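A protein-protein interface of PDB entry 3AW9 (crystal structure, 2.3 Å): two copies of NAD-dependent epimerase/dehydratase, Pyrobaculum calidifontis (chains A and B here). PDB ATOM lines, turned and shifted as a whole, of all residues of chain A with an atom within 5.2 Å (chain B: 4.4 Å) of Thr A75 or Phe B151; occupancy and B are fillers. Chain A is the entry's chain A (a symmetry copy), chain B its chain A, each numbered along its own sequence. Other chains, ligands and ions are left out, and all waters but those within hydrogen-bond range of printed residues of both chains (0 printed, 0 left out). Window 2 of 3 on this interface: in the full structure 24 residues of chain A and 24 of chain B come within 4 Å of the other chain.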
ATOM      1  N   VAL A  71     -14.264 -16.540 -19.265  1.00  0.00           N
ATOM      2  CA  VAL A  71     -14.327 -16.263 -20.722  1.00  0.00           C
ATOM      3  C   VAL A  71     -13.917 -14.818 -21.075  1.00  0.00           C
ATOM      4  O   VAL A  71     -13.440 -14.530 -22.172  1.00  0.00           O
ATOM      5  CB  VAL A  71     -15.761 -16.567 -21.292  1.00  0.00           C
ATOM      6  CG1 VAL A  71     -15.891 -16.171 -22.765  1.00  0.00           C
ATOM      7  CG2 VAL A  71     -16.129 -18.038 -21.112  1.00  0.00           C
ATOM      8  N   ARG A  72     -14.102 -13.910 -20.132  1.00  0.00           N
ATOM      9  CA  ARG A  72     -13.958 -12.505 -20.412  1.00  0.00           C
ATOM     10  C   ARG A  72     -12.493 -12.079 -20.485  1.00  0.00           C
ATOM     11  O   ARG A  72     -12.099 -11.317 -21.375  1.00  0.00           O
ATOM     12  CB  ARG A  72     -14.689 -11.730 -19.334  1.00  0.00           C
ATOM     13  CG  ARG A  72     -15.289 -10.447 -19.812  1.00  0.00           C
ATOM     14  CD  ARG A  72     -15.741  -9.641 -18.624  1.00  0.00           C
ATOM     15  NE  ARG A  72     -16.512 -10.466 -17.700  1.00  0.00           N
ATOM     16  CZ  ARG A  72     -17.287  -9.985 -16.738  1.00  0.00           C
ATOM     17  NH1 ARG A  72     -17.403  -8.667 -16.575  1.00  0.00           N
ATOM     18  NH2 ARG A  72     -17.954 -10.826 -15.953  1.00  0.00           N
ATOM     19  N   THR A  75      -9.721 -12.497 -24.770  1.00  0.00           N
ATOM     20  CA  THR A  75      -9.765 -11.287 -25.602  1.00  0.00           C
ATOM     21  C   THR A  75      -8.668 -10.296 -25.192  1.00  0.00           C
ATOM     22  O   THR A  75      -7.885  -9.822 -26.038  1.00  0.00           O
ATOM     23  CB  THR A  75     -11.160 -10.554 -25.541  1.00  0.00           C
ATOM     24  OG1 THR A  75     -12.235 -11.500 -25.630  1.00  0.00           O
ATOM     25  CG2 THR A  75     -11.304  -9.524 -26.658  1.00  0.00           C
ATOM     26  N   THR A  76      -8.628  -9.980 -23.895  1.00  0.00           N
ATOM     27  CA  THR A  76      -7.734  -8.938 -23.382  1.00  0.00           C
ATOM     28  C   THR A  76      -6.406  -9.515 -22.916  1.00  0.00           C
ATOM     29  O   THR A  76      -5.357  -8.879 -23.074  1.00  0.00           O
ATOM     30  CB  THR A  76      -8.384  -8.099 -22.235  1.00  0.00           C
ATOM     31  OG1 THR A  76      -8.463  -8.884 -21.036  1.00  0.00           O
ATOM     32  CG2 THR A  76      -9.778  -7.594 -22.632  1.00  0.00           C
ATOM     33  N   GLU A  77      -6.451 -10.721 -22.349  1.00  0.00           N
ATOM     34  CA  GLU A  77      -5.229 -11.400 -21.898  1.00  0.00           C
ATOM     35  C   GLU A  77      -5.100 -12.902 -22.320  1.00  0.00           C
ATOM     36  O   GLU A  77      -4.962 -13.784 -21.456  1.00  0.00           O
ATOM     37  CB  GLU A  77      -5.074 -11.214 -20.389  1.00  0.00           C
ATOM     38  CG  GLU A  77      -3.657 -10.875 -19.978  1.00  0.00           C
ATOM     39  CD  GLU A  77      -3.453 -10.980 -18.475  1.00  0.00           C
ATOM     40  OE1 GLU A  77      -2.283 -10.873 -18.021  1.00  0.00           O
ATOM     41  OE2 GLU A  77      -4.467 -11.180 -17.755  1.00  0.00           O
ATOM     42  N   PRO A  78      -5.137 -13.186 -23.653  1.00  0.00           N
ATOM     43  CA  PRO A  78      -5.199 -14.571 -24.183  1.00  0.00           C
ATOM     44  C   PRO A  78      -4.049 -15.511 -23.755  1.00  0.00           C
ATOM     45  O   PRO A  78      -4.238 -16.735 -23.772  1.00  0.00           O
ATOM     46  CB  PRO A  78      -5.191 -14.373 -25.711  1.00  0.00           C
ATOM     47  CG  PRO A  78      -5.702 -12.964 -25.923  1.00  0.00           C
ATOM     48  CD  PRO A  78      -5.153 -12.191 -24.748  1.00  0.00           C
ATOM     49  N   HIS A  81      -4.942 -17.332 -20.568  1.00  0.00           N
ATOM     50  CA  HIS A  81      -5.764 -18.435 -21.037  1.00  0.00           C
ATOM     51  C   HIS A  81      -4.931 -19.522 -21.685  1.00  0.00           C
ATOM     52  O   HIS A  81      -5.295 -20.702 -21.604  1.00  0.00           O
ATOM     53  CB  HIS A  81      -6.833 -18.000 -22.043  1.00  0.00           C
ATOM     54  CG  HIS A  81      -8.066 -17.426 -21.419  1.00  0.00           C
ATOM     55  ND1 HIS A  81      -8.902 -16.564 -22.095  1.00  0.00           N
ATOM     56  CD2 HIS A  81      -8.582 -17.554 -20.169  1.00  0.00           C
ATOM     57  CE1 HIS A  81      -9.891 -16.200 -21.294  1.00  0.00           C
ATOM     58  NE2 HIS A  81      -9.724 -16.794 -20.122  1.00  0.00           N
ATOM     59  N   VAL A 132     -11.202 -17.231 -26.845  1.00  0.00           N
ATOM     60  CA  VAL A 132      -9.907 -17.877 -26.685  1.00  0.00           C
ATOM     61  C   VAL A 132      -9.981 -19.040 -25.684  1.00  0.00           C
ATOM     62  O   VAL A 132      -9.302 -20.038 -25.834  1.00  0.00           O
ATOM     63  CB  VAL A 132      -8.783 -16.815 -26.354  1.00  0.00           C
ATOM     64  CG1 VAL A 132      -7.439 -17.473 -25.996  1.00  0.00           C
ATOM     65  CG2 VAL A 132      -8.586 -15.862 -27.565  1.00  0.00           C
ATOM     66  N   PRO A 266     -16.974  -9.192 -26.374  1.00  0.00           N
ATOM     67  CA  PRO A 266     -16.600  -9.990 -27.562  1.00  0.00           C
ATOM     68  C   PRO A 266     -16.258 -11.439 -27.193  1.00  0.00           C
ATOM     69  O   PRO A 266     -15.464 -11.679 -26.274  1.00  0.00           O
ATOM     70  CB  PRO A 266     -15.383  -9.225 -28.143  1.00  0.00           C
ATOM     71  CG  PRO A 266     -15.593  -7.778 -27.656  1.00  0.00           C
ATOM     72  CD  PRO A 266     -16.096  -8.010 -26.223  1.00  0.00           C
ATOM     73  N   ARG B  97      -2.748 -10.297 -34.215  1.00  0.00           N
ATOM     74  CA  ARG B  97      -3.723  -9.501 -33.489  1.00  0.00           C
ATOM     75  C   ARG B  97      -3.230  -8.080 -33.101  1.00  0.00           C
ATOM     76  O   ARG B  97      -3.892  -7.090 -33.389  1.00  0.00           O
ATOM     77  CB  ARG B  97      -4.198 -10.247 -32.237  1.00  0.00           C
ATOM     78  CG  ARG B  97      -5.147  -9.409 -31.377  1.00  0.00           C
ATOM     79  CD  ARG B  97      -5.640 -10.163 -30.165  1.00  0.00           C
ATOM     80  NE  ARG B  97      -4.611 -10.354 -29.151  1.00  0.00           N
ATOM     81  CZ  ARG B  97      -4.288  -9.423 -28.260  1.00  0.00           C
ATOM     82  NH1 ARG B  97      -4.911  -8.249 -28.286  1.00  0.00           N
ATOM     83  NH2 ARG B  97      -3.353  -9.660 -27.354  1.00  0.00           N
ATOM     84  N   TYR B 147      -9.376 -16.604 -33.645  1.00  0.00           N
ATOM     85  CA  TYR B 147      -8.836 -15.274 -33.843  1.00  0.00           C
ATOM     86  C   TYR B 147      -9.526 -14.556 -34.999  1.00  0.00           C
ATOM     87  O   TYR B 147      -9.690 -13.340 -34.947  1.00  0.00           O
ATOM     88  CB  TYR B 147      -7.303 -15.310 -34.052  1.00  0.00           C
ATOM     89  CG  TYR B 147      -6.541 -15.245 -32.746  1.00  0.00           C
ATOM     90  CD1 TYR B 147      -6.692 -16.237 -31.766  1.00  0.00           C
ATOM     91  CD2 TYR B 147      -5.692 -14.191 -32.479  1.00  0.00           C
ATOM     92  CE1 TYR B 147      -5.986 -16.178 -30.556  1.00  0.00           C
ATOM     93  CE2 TYR B 147      -4.987 -14.112 -31.268  1.00  0.00           C
ATOM     94  CZ  TYR B 147      -5.143 -15.103 -30.317  1.00  0.00           C
ATOM     95  OH  TYR B 147      -4.459 -14.982 -29.142  1.00  0.00           O
ATOM     96  N   ALA B 148      -9.905 -15.314 -36.029  1.00  0.00           N
ATOM     97  CA  ALA B 148     -10.702 -14.788 -37.161  1.00  0.00           C
ATOM     98  C   ALA B 148     -12.045 -14.266 -36.714  1.00  0.00           C
ATOM     99  O   ALA B 148     -12.424 -13.169 -37.071  1.00  0.00           O
ATOM    100  CB  ALA B 148     -10.907 -15.833 -38.238  1.00  0.00           C
ATOM    101  N   ARG B 149     -12.759 -15.071 -35.946  1.00  0.00           N
ATOM    102  CA  ARG B 149     -14.123 -14.756 -35.564  1.00  0.00           C
ATOM    103  C   ARG B 149     -14.146 -13.617 -34.544  1.00  0.00           C
ATOM    104  O   ARG B 149     -15.005 -12.740 -34.600  1.00  0.00           O
ATOM    105  CB  ARG B 149     -14.808 -16.015 -35.025  1.00  0.00           C
ATOM    106  CG  ARG B 149     -15.033 -17.091 -36.102  1.00  0.00           C
ATOM    107  CD  ARG B 149     -15.936 -18.225 -35.622  1.00  0.00           C
ATOM    108  NE  ARG B 149     -15.180 -19.220 -34.883  1.00  0.00           N
ATOM    109  CZ  ARG B 149     -14.670 -20.352 -35.381  1.00  0.00           C
ATOM    110  NH1 ARG B 149     -14.835 -20.706 -36.652  1.00  0.00           N
ATOM    111  NH2 ARG B 149     -13.987 -21.147 -34.578  1.00  0.00           N
ATOM    112  N   LEU B 150     -13.162 -13.611 -33.644  1.00  0.00           N
ATOM    113  CA  LEU B 150     -13.126 -12.704 -32.511  1.00  0.00           C
ATOM    114  C   LEU B 150     -12.460 -11.377 -32.835  1.00  0.00           C
ATOM    115  O   LEU B 150     -12.983 -10.308 -32.480  1.00  0.00           O
ATOM    116  CB  LEU B 150     -12.421 -13.402 -31.338  1.00  0.00           C
ATOM    117  CG  LEU B 150     -12.376 -12.735 -29.976  1.00  0.00           C
ATOM    118  CD1 LEU B 150     -13.776 -12.333 -29.502  1.00  0.00           C
ATOM    119  CD2 LEU B 150     -11.647 -13.641 -28.946  1.00  0.00           C
ATOM    120  N   PHE B 151     -11.324 -11.427 -33.526  1.00  0.00           N
ATOM    121  CA  PHE B 151     -10.541 -10.204 -33.777  1.00  0.00           C
ATOM    122  C   PHE B 151     -10.535  -9.757 -35.235  1.00  0.00           C
ATOM    123  O   PHE B 151      -9.878  -8.783 -35.578  1.00  0.00           O
ATOM    124  CB  PHE B 151      -9.099 -10.373 -33.298  1.00  0.00           C
ATOM    125  CG  PHE B 151      -8.974 -10.784 -31.850  1.00  0.00           C
ATOM    126  CD1 PHE B 151      -9.434  -9.948 -30.816  1.00  0.00           C
ATOM    127  CD2 PHE B 151      -8.391 -12.004 -31.516  1.00  0.00           C
ATOM    128  CE1 PHE B 151      -9.297 -10.345 -29.458  1.00  0.00           C
ATOM    129  CE2 PHE B 151      -8.245 -12.406 -30.166  1.00  0.00           C
ATOM    130  CZ  PHE B 151      -8.694 -11.584 -29.141  1.00  0.00           C
ATOM    131  N   GLY B 152     -11.221 -10.496 -36.096  1.00  0.00           N
ATOM    132  CA  GLY B 152     -11.169 -10.219 -37.516  1.00  0.00           C
ATOM    133  C   GLY B 152      -9.885 -10.552 -38.249  1.00  0.00           C
ATOM    134  O   GLY B 152      -9.726 -10.140 -39.404  1.00  0.00           O
ATOM    135  N   VAL B 153      -8.957 -11.261 -37.597  1.00  0.00           N
ATOM    136  CA  VAL B 153      -7.755 -11.766 -38.277  1.00  0.00           C
ATOM    137  C   VAL B 153      -8.173 -13.024 -39.070  1.00  0.00           C
ATOM    138  O   VAL B 153      -8.056 -14.164 -38.577  1.00  0.00           O
ATOM    139  CB  VAL B 153      -6.589 -12.088 -37.296  1.00  0.00           C
ATOM    140  CG1 VAL B 153      -5.284 -12.356 -38.062  1.00  0.00           C
ATOM    141  CG2 VAL B 153      -6.371 -10.975 -36.243  1.00  0.00           C
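The backbone carbonyl oxygen of Tyr B147 sits at hydrogen-bond distance from the backbone NH of Val B153, 3.4 Å away. The side-chain hydroxyl of Thr A75 lies within hydrogen-bond range of the backbone carbonyl oxygen of Pro A266, 3.3 Å away. The backbone carbonyl oxygen (O) of Tyr B147 sits at hydrogen-bond distance from the backbone NH (N) of Gly B152 (3.4 Å).
Printed residues of chain B within 4 Å of Thr A75: Leu B150 and Phe B151. Phe B151 touches one residue of chain A. Of the printed residues of chain A, Tyr B147 touches Pro A78 and Val A132. Of the printed residues of chain A, Leu B150 touches Thr A75 (3.99 Å) and Pro A266 (3.5 Å). Of the printed residues of chain B, Pro A266 touches Leu B150. The nearest printed residue of chain A that does not touch Tyr B147 is Thr A75 (6.9 Å).
Hydrophobic or aromatic side chains of chain A that line the printed part of chain B: Pro A78, Val A132 and Pro A266. Of the 8 printed residues of chain B, 3 touch a printed residue of chain A. Hydrophobic or aromatic side chains of chain B within 4 Å of the printed part of chain A: Tyr B147, Leu B150 and Phe B151. Along chain B the printed residues that touch a printed residue of chain A span positions 147 to 151.
Leu B150 touches Thr A75 (CD2 to OG1, 3.99 Å). CG2 of Thr A75 touches CE1 of Phe B151, 3.5 Å away. Tyr B147 touches Pro A78 (OH to CB, 3.6 Å). Tyr B147 touches Val A132 (CE1 to CG2, 3.98 Å). Leu B150 touches Pro A266.
No position is printed for both chains.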
